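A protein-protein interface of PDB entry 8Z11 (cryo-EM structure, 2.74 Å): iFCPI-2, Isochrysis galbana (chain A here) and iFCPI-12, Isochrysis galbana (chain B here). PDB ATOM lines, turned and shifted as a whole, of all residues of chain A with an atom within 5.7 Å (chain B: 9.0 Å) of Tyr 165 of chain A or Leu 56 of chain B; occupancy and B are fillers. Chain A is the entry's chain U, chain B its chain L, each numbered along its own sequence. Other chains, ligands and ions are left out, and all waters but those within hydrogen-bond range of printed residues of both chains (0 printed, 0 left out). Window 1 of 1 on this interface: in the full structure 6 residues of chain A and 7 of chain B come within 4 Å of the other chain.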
ATOM      1  N   MET A 155      21.727 -19.296   6.254  1.00  0.00           N
ATOM      2  CA  MET A 155      20.404 -18.893   5.781  1.00  0.00           C
ATOM      3  C   MET A 155      19.926 -17.652   6.538  1.00  0.00           C
ATOM      4  O   MET A 155      18.756 -17.525   6.899  1.00  0.00           O
ATOM      5  CB  MET A 155      19.401 -20.053   5.883  1.00  0.00           C
ATOM      6  CG  MET A 155      18.440 -20.199   4.676  1.00  0.00           C
ATOM      7  SD  MET A 155      19.102 -20.912   3.140  1.00  0.00           S
ATOM      8  CE  MET A 155      19.378 -22.624   3.617  1.00  0.00           C
ATOM      9  N   LEU A 156      20.862 -16.730   6.786  1.00  0.00           N
ATOM     10  CA  LEU A 156      20.523 -15.443   7.386  1.00  0.00           C
ATOM     11  C   LEU A 156      19.795 -14.538   6.400  1.00  0.00           C
ATOM     12  O   LEU A 156      19.159 -13.560   6.812  1.00  0.00           O
ATOM     13  CB  LEU A 156      21.791 -14.744   7.886  1.00  0.00           C
ATOM     14  CG  LEU A 156      22.736 -15.553   8.787  1.00  0.00           C
ATOM     15  CD1 LEU A 156      23.894 -14.717   9.371  1.00  0.00           C
ATOM     16  CD2 LEU A 156      21.958 -16.230   9.904  1.00  0.00           C
ATOM     17  N   LEU A 157      19.906 -14.819   5.099  1.00  0.00           N
ATOM     18  CA  LEU A 157      19.174 -14.067   4.090  1.00  0.00           C
ATOM     19  C   LEU A 157      17.705 -14.459   4.010  1.00  0.00           C
ATOM     20  O   LEU A 157      16.937 -13.762   3.339  1.00  0.00           O
ATOM     21  CB  LEU A 157      19.828 -14.262   2.722  1.00  0.00           C
ATOM     22  CG  LEU A 157      21.225 -13.662   2.551  1.00  0.00           C
ATOM     23  CD1 LEU A 157      21.901 -14.221   1.304  1.00  0.00           C
ATOM     24  CD2 LEU A 157      21.175 -12.142   2.505  1.00  0.00           C
ATOM     25  N   SER A 159      15.839 -14.136   6.492  1.00  0.00           N
ATOM     26  CA  SER A 159      15.233 -13.334   7.542  1.00  0.00           C
ATOM     27  C   SER A 159      14.203 -12.400   6.923  1.00  0.00           C
ATOM     28  O   SER A 159      14.264 -12.130   5.717  1.00  0.00           O
ATOM     29  CB  SER A 159      16.293 -12.519   8.285  1.00  0.00           C
ATOM     30  OG  SER A 159      16.537 -11.286   7.632  1.00  0.00           O
ATOM     31  N   ASN A 161      14.283  -9.357   7.243  1.00  0.00           N
ATOM     32  CA  ASN A 161      15.083  -8.168   6.948  1.00  0.00           C
ATOM     33  C   ASN A 161      16.442  -8.571   6.362  1.00  0.00           C
ATOM     34  O   ASN A 161      17.465  -8.568   7.047  1.00  0.00           O
ATOM     35  CB  ASN A 161      15.203  -7.310   8.222  1.00  0.00           C
ATOM     36  CG  ASN A 161      15.715  -8.090   9.433  1.00  0.00           C
ATOM     37  OD1 ASN A 161      16.427  -9.085   9.312  1.00  0.00           O
ATOM     38  ND2 ASN A 161      15.333  -7.633  10.619  1.00  0.00           N
ATOM     39  N   ALA A 162      16.450  -8.859   5.057  1.00  0.00           N
ATOM     40  CA  ALA A 162      17.666  -9.195   4.320  1.00  0.00           C
ATOM     41  C   ALA A 162      18.184  -8.050   3.465  1.00  0.00           C
ATOM     42  O   ALA A 162      19.402  -7.911   3.301  1.00  0.00           O
ATOM     43  CB  ALA A 162      17.425 -10.415   3.419  1.00  0.00           C
ATOM     44  N   GLU A 163      17.287  -7.226   2.914  1.00  0.00           N
ATOM     45  CA  GLU A 163      17.717  -5.960   2.332  1.00  0.00           C
ATOM     46  C   GLU A 163      18.440  -5.112   3.370  1.00  0.00           C
ATOM     47  O   GLU A 163      19.397  -4.401   3.041  1.00  0.00           O
ATOM     48  CB  GLU A 163      16.516  -5.193   1.773  1.00  0.00           C
ATOM     49  CG  GLU A 163      15.679  -5.936   0.730  1.00  0.00           C
ATOM     50  CD  GLU A 163      14.438  -5.157   0.331  1.00  0.00           C
ATOM     51  OE1 GLU A 163      14.298  -3.997   0.770  1.00  0.00           O
ATOM     52  OE2 GLU A 163      13.601  -5.703  -0.419  1.00  0.00           O
ATOM     53  N   LYS A 164      17.995  -5.186   4.630  1.00  0.00           N
ATOM     54  CA  LYS A 164      18.710  -4.545   5.726  1.00  0.00           C
ATOM     55  C   LYS A 164      20.143  -5.055   5.821  1.00  0.00           C
ATOM     56  O   LYS A 164      21.073  -4.264   5.992  1.00  0.00           O
ATOM     57  CB  LYS A 164      17.945  -4.782   7.035  1.00  0.00           C
ATOM     58  CG  LYS A 164      18.611  -4.300   8.359  1.00  0.00           C
ATOM     59  CD  LYS A 164      18.047  -5.050   9.585  1.00  0.00           C
ATOM     60  CE  LYS A 164      19.096  -5.400  10.638  1.00  0.00           C
ATOM     61  NZ  LYS A 164      20.080  -4.327  10.948  1.00  0.00           N
ATOM     62  N   TYR A 165      20.342  -6.372   5.731  1.00  0.00           N
ATOM     63  CA  TYR A 165      21.697  -6.910   5.814  1.00  0.00           C
ATOM     64  C   TYR A 165      22.546  -6.457   4.639  1.00  0.00           C
ATOM     65  O   TYR A 165      23.726  -6.130   4.809  1.00  0.00           O
ATOM     66  CB  TYR A 165      21.664  -8.438   5.875  1.00  0.00           C
ATOM     67  CG  TYR A 165      21.103  -9.049   7.146  1.00  0.00           C
ATOM     68  CD1 TYR A 165      20.842  -8.282   8.280  1.00  0.00           C
ATOM     69  CD2 TYR A 165      20.859 -10.411   7.214  1.00  0.00           C
ATOM     70  CE1 TYR A 165      20.347  -8.853   9.423  1.00  0.00           C
ATOM     71  CE2 TYR A 165      20.363 -10.987   8.355  1.00  0.00           C
ATOM     72  CZ  TYR A 165      20.111 -10.204   9.455  1.00  0.00           C
ATOM     73  OH  TYR A 165      19.618 -10.782  10.591  1.00  0.00           O
ATOM     74  N   LYS A 166      21.972  -6.447   3.437  1.00  0.00           N
ATOM     75  CA  LYS A 166      22.727  -6.005   2.267  1.00  0.00           C
ATOM     76  C   LYS A 166      23.157  -4.549   2.424  1.00  0.00           C
ATOM     77  O   LYS A 166      24.328  -4.197   2.207  1.00  0.00           O
ATOM     78  CB  LYS A 166      21.891  -6.191   1.000  1.00  0.00           C
ATOM     79  CG  LYS A 166      21.295  -7.587   0.832  1.00  0.00           C
ATOM     80  CD  LYS A 166      21.536  -8.162  -0.554  1.00  0.00           C
ATOM     81  CE  LYS A 166      22.960  -8.663  -0.719  1.00  0.00           C
ATOM     82  NZ  LYS A 166      23.165  -9.321  -2.039  1.00  0.00           N
ATOM     83  N   LEU A 167      22.221  -3.689   2.836  1.00  0.00           N
ATOM     84  CA  LEU A 167      22.546  -2.284   3.044  1.00  0.00           C
ATOM     85  C   LEU A 167      23.579  -2.115   4.149  1.00  0.00           C
ATOM     86  O   LEU A 167      24.495  -1.293   4.030  1.00  0.00           O
ATOM     87  CB  LEU A 167      21.274  -1.501   3.368  1.00  0.00           C
ATOM     88  CG  LEU A 167      21.409   0.021   3.479  1.00  0.00           C
ATOM     89  CD1 LEU A 167      20.179   0.694   2.890  1.00  0.00           C
ATOM     90  CD2 LEU A 167      21.616   0.479   4.924  1.00  0.00           C
ATOM     91  N   ALA A 168      23.439  -2.871   5.240  1.00  0.00           N
ATOM     92  CA  ALA A 168      24.388  -2.763   6.340  1.00  0.00           C
ATOM     93  C   ALA A 168      25.783  -3.155   5.884  1.00  0.00           C
ATOM     94  O   ALA A 168      26.763  -2.487   6.227  1.00  0.00           O
ATOM     95  CB  ALA A 168      23.941  -3.633   7.514  1.00  0.00           C
ATOM     96  N   GLU A 169      25.886  -4.220   5.087  1.00  0.00           N
ATOM     97  CA  GLU A 169      27.170  -4.602   4.510  1.00  0.00           C
ATOM     98  C   GLU A 169      27.757  -3.458   3.695  1.00  0.00           C
ATOM     99  O   GLU A 169      28.935  -3.116   3.847  1.00  0.00           O
ATOM    100  CB  GLU A 169      27.006  -5.849   3.642  1.00  0.00           C
ATOM    101  CG  GLU A 169      28.314  -6.555   3.313  1.00  0.00           C
ATOM    102  CD  GLU A 169      28.118  -7.781   2.440  1.00  0.00           C
ATOM    103  OE1 GLU A 169      27.171  -7.790   1.627  1.00  0.00           O
ATOM    104  OE2 GLU A 169      28.912  -8.737   2.568  1.00  0.00           O
ATOM    105  N   LEU A 170      26.936  -2.828   2.851  1.00  0.00           N
ATOM    106  CA  LEU A 170      27.452  -1.769   1.982  1.00  0.00           C
ATOM    107  C   LEU A 170      27.966  -0.575   2.787  1.00  0.00           C
ATOM    108  O   LEU A 170      29.111  -0.134   2.602  1.00  0.00           O
ATOM    109  CB  LEU A 170      26.376  -1.325   0.988  1.00  0.00           C
ATOM    110  CG  LEU A 170      26.438  -1.926  -0.422  1.00  0.00           C
ATOM    111  CD1 LEU A 170      27.659  -1.425  -1.188  1.00  0.00           C
ATOM    112  CD2 LEU A 170      26.425  -3.449  -0.381  1.00  0.00           C
ATOM    113  N   ASP B  49      14.592 -14.611  24.610  1.00  0.00           N
ATOM    114  CA  ASP B  49      15.506 -14.085  23.596  1.00  0.00           C
ATOM    115  C   ASP B  49      15.534 -12.564  23.719  1.00  0.00           C
ATOM    116  O   ASP B  49      14.934 -11.855  22.899  1.00  0.00           O
ATOM    117  CB  ASP B  49      15.089 -14.537  22.195  1.00  0.00           C
ATOM    118  CG  ASP B  49      16.156 -14.265  21.150  1.00  0.00           C
ATOM    119  OD1 ASP B  49      17.242 -13.766  21.513  1.00  0.00           O
ATOM    120  OD2 ASP B  49      15.908 -14.550  19.960  1.00  0.00           O
ATOM    121  N   LEU B  51      18.047 -10.328  23.147  1.00  0.00           N
ATOM    122  CA  LEU B  51      18.629  -9.739  21.948  1.00  0.00           C
ATOM    123  C   LEU B  51      17.865 -10.098  20.681  1.00  0.00           C
ATOM    124  O   LEU B  51      18.156  -9.529  19.622  1.00  0.00           O
ATOM    125  CB  LEU B  51      20.094 -10.169  21.796  1.00  0.00           C
ATOM    126  CG  LEU B  51      21.164  -9.411  22.594  1.00  0.00           C
ATOM    127  CD1 LEU B  51      21.231  -7.934  22.209  1.00  0.00           C
ATOM    128  CD2 LEU B  51      20.931  -9.561  24.089  1.00  0.00           C
ATOM    129  N   GLY B  52      16.907 -11.016  20.755  1.00  0.00           N
ATOM    130  CA  GLY B  52      16.107 -11.359  19.595  1.00  0.00           C
ATOM    131  C   GLY B  52      16.910 -12.014  18.495  1.00  0.00           C
ATOM    132  O   GLY B  52      16.622 -11.797  17.311  1.00  0.00           O
ATOM    133  N   LEU B  53      17.912 -12.821  18.853  1.00  0.00           N
ATOM    134  CA  LEU B  53      18.756 -13.423  17.830  1.00  0.00           C
ATOM    135  C   LEU B  53      18.057 -14.520  17.045  1.00  0.00           C
ATOM    136  O   LEU B  53      18.588 -14.940  16.013  1.00  0.00           O
ATOM    137  CB  LEU B  53      20.046 -13.990  18.425  1.00  0.00           C
ATOM    138  CG  LEU B  53      20.916 -13.039  19.244  1.00  0.00           C
ATOM    139  CD1 LEU B  53      21.063 -13.555  20.659  1.00  0.00           C
ATOM    140  CD2 LEU B  53      22.275 -12.848  18.589  1.00  0.00           C
ATOM    141  N   ALA B  54      16.899 -15.003  17.502  1.00  0.00           N
ATOM    142  CA  ALA B  54      16.150 -15.981  16.721  1.00  0.00           C
ATOM    143  C   ALA B  54      15.682 -15.417  15.386  1.00  0.00           C
ATOM    144  O   ALA B  54      15.390 -16.191  14.469  1.00  0.00           O
ATOM    145  CB  ALA B  54      14.948 -16.479  17.525  1.00  0.00           C
ATOM    146  N   SER B  55      15.608 -14.093  15.254  1.00  0.00           N
ATOM    147  CA  SER B  55      15.123 -13.438  14.049  1.00  0.00           C
ATOM    148  C   SER B  55      16.235 -13.071  13.071  1.00  0.00           C
ATOM    149  O   SER B  55      15.960 -12.394  12.075  1.00  0.00           O
ATOM    150  CB  SER B  55      14.334 -12.182  14.425  1.00  0.00           C
ATOM    151  OG  SER B  55      13.193 -12.514  15.195  1.00  0.00           O
ATOM    152  N   LEU B  56      17.482 -13.486  13.321  1.00  0.00           N
ATOM    153  CA  LEU B  56      18.528 -13.239  12.334  1.00  0.00           C
ATOM    154  C   LEU B  56      18.274 -13.952  11.015  1.00  0.00           C
ATOM    155  O   LEU B  56      18.838 -13.550   9.991  1.00  0.00           O
ATOM    156  CB  LEU B  56      19.910 -13.652  12.848  1.00  0.00           C
ATOM    157  CG  LEU B  56      20.765 -12.579  13.525  1.00  0.00           C
ATOM    158  CD1 LEU B  56      20.259 -12.230  14.890  1.00  0.00           C
ATOM    159  CD2 LEU B  56      22.210 -13.044  13.590  1.00  0.00           C
ATOM    160  N   GLY B  57      17.464 -15.006  11.014  1.00  0.00           N
ATOM    161  CA  GLY B  57      17.173 -15.748   9.805  1.00  0.00           C
ATOM    162  C   GLY B  57      15.841 -16.458   9.896  1.00  0.00           C
ATOM    163  O   GLY B  57      14.988 -16.087  10.707  1.00  0.00           O
ATOM    164  N   GLY B  58      15.651 -17.483   9.074  1.00  0.00           N
ATOM    165  CA  GLY B  58      14.441 -18.280   9.106  1.00  0.00           C
ATOM    166  C   GLY B  58      14.526 -19.360  10.160  1.00  0.00           C
ATOM    167  O   GLY B  58      15.244 -19.237  11.158  1.00  0.00           O
ATOM    168  N   GLU B  59      13.774 -20.437   9.943  1.00  0.00           N
ATOM    169  CA  GLU B  59      13.859 -21.585  10.833  1.00  0.00           C
ATOM    170  C   GLU B  59      15.210 -22.282  10.728  1.00  0.00           C
ATOM    171  O   GLU B  59      15.611 -22.976  11.668  1.00  0.00           O
ATOM    172  CB  GLU B  59      12.714 -22.557  10.520  1.00  0.00           C
ATOM    173  CG  GLU B  59      12.750 -23.892  11.263  1.00  0.00           C
ATOM    174  CD  GLU B  59      12.760 -23.722  12.770  1.00  0.00           C
ATOM    175  OE1 GLU B  59      11.709 -23.354  13.335  1.00  0.00           O
ATOM    176  OE2 GLU B  59      13.818 -23.958  13.391  1.00  0.00           O
ATOM    177  N   GLU B  60      15.928 -22.095   9.617  1.00  0.00           N
ATOM    178  CA  GLU B  60      17.194 -22.795   9.417  1.00  0.00           C
ATOM    179  C   GLU B  60      18.248 -22.315  10.405  1.00  0.00           C
ATOM    180  O   GLU B  60      18.958 -23.124  11.015  1.00  0.00           O
ATOM    181  CB  GLU B  60      17.689 -22.613   7.976  1.00  0.00           C
ATOM    182  CG  GLU B  60      16.907 -23.339   6.854  1.00  0.00           C
ATOM    183  CD  GLU B  60      15.414 -23.051   6.821  1.00  0.00           C
ATOM    184  OE1 GLU B  60      14.694 -23.719   6.050  1.00  0.00           O
ATOM    185  OE2 GLU B  60      14.959 -22.154   7.560  1.00  0.00           O
ATOM    186  N   THR B  61      18.368 -20.996  10.583  1.00  0.00           N
ATOM    187  CA  THR B  61      19.365 -20.486  11.515  1.00  0.00           C
ATOM    188  C   THR B  61      19.008 -20.834  12.954  1.00  0.00           C
ATOM    189  O   THR B  61      19.905 -21.055  13.773  1.00  0.00           O
ATOM    190  CB  THR B  61      19.543 -18.973  11.347  1.00  0.00           C
ATOM    191  OG1 THR B  61      20.844 -18.591  11.809  1.00  0.00           O
ATOM    192  CG2 THR B  61      18.492 -18.179  12.115  1.00  0.00           C
ATOM    193  N   LEU B  62      17.718 -20.902  13.283  1.00  0.00           N
ATOM    194  CA  LEU B  62      17.330 -21.284  14.636  1.00  0.00           C
ATOM    195  C   LEU B  62      17.609 -22.760  14.884  1.00  0.00           C
ATOM    196  O   LEU B  62      18.022 -23.143  15.984  1.00  0.00           O
ATOM    197  CB  LEU B  62      15.854 -20.963  14.869  1.00  0.00           C
ATOM    198  CG  LEU B  62      15.363 -20.892  16.317  1.00  0.00           C
ATOM    199  CD1 LEU B  62      16.078 -19.806  17.115  1.00  0.00           C
ATOM    200  CD2 LEU B  62      13.863 -20.662  16.342  1.00  0.00           C
ATOM    201  N   PHE B  65      21.258 -22.882  15.503  1.00  0.00           N
ATOM    202  CA  PHE B  65      21.567 -22.405  16.845  1.00  0.00           C
ATOM    203  C   PHE B  65      21.232 -23.460  17.890  1.00  0.00           C
ATOM    204  O   PHE B  65      21.983 -23.647  18.853  1.00  0.00           O
ATOM    205  CB  PHE B  65      20.802 -21.109  17.139  1.00  0.00           C
ATOM    206  CG  PHE B  65      21.267 -19.894  16.350  1.00  0.00           C
ATOM    207  CD1 PHE B  65      22.312 -19.950  15.433  1.00  0.00           C
ATOM    208  CD2 PHE B  65      20.640 -18.677  16.548  1.00  0.00           C
ATOM    209  CE1 PHE B  65      22.705 -18.827  14.740  1.00  0.00           C
ATOM    210  CE2 PHE B  65      21.032 -17.554  15.856  1.00  0.00           C
ATOM    211  CZ  PHE B  65      22.067 -17.629  14.952  1.00  0.00           C
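Among the printed residues, pairs that only touch across the chains: Met 155 of chain A with Gly 57 of chain B (3.8 Å), Met 155 of chain A with Gly 58 of chain B (3.8 Å), Met 155 of chain A with Glu 60 of chain B (3.7 Å), Leu 156 of chain A with Thr 61 of chain B (3.2 Å), Ser 159 of chain A with Ser 55 of chain B (3.8 Å), Ser 159 of chain A with Leu 56 of chain B (3.2 Å) and Ser 159 of chain A with Gly 57 of chain B (3.7 Å).
Tyr 165 of chain A touches just one residue of chain B: Leu 56.
Of chain A, only Leu 156, Ser 159 and Tyr 165 come within 4 Å of Leu 56 of chain B.
Leu 156 of chain A touches just these residues of chain B: Leu 56 (3.2 Å) and Thr 61 (3.2 Å).
Lys 164 of chain A touches none of the printed residues of chain B.
Of the printed residues of chain A, Gly 57 of chain B touches Met 155 and Ser 159.
Printed residues of chain A within 4 Å of Gly 58 of chain B: Met 155 (3.8 Å).
Printed residues of chain B within 4 Å of Met 155 of chain A: Gly 57 (3.8 Å), Gly 58 (3.8 Å) and Glu 60 (3.7 Å).
Gly 52 of chain B touches none of the printed residues of chain A.
The nearest printed residue of chain A that does not touch Gly 58 of chain B is Ser 159 of chain A (4.2 Å).
Of the 14 printed residues of chain A, 4 touch a printed residue of chain B.
Printed residues of chain B that touch a printed residue of chain A: Ser 55, Leu 56, Gly 57, Gly 58, Glu 60 and Thr 61.
Hydrophobic or aromatic side chains of chain B that line the printed part of chain A: Leu 56.
Along chain B the printed residues that touch a printed residue of chain A span positions 55 to 61.
The backbone carbonyl oxygen (O) of Leu 156 of chain A sits close to the backbone carbonyl oxygen (O) of Leu 56 of chain B.
The backbone carbonyl oxygen (O) of Leu 56 of chain B is in hydrogen-bond range of the side-chain hydroxyl (OH) of Tyr 165 of chain A (2.9 Å).
The side-chain amide oxygen (OD1) of Asn 161 of chain A sits at hydrogen-bond distance from the side-chain hydroxyl (OG) of Ser 159 of chain A (2.8 Å).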
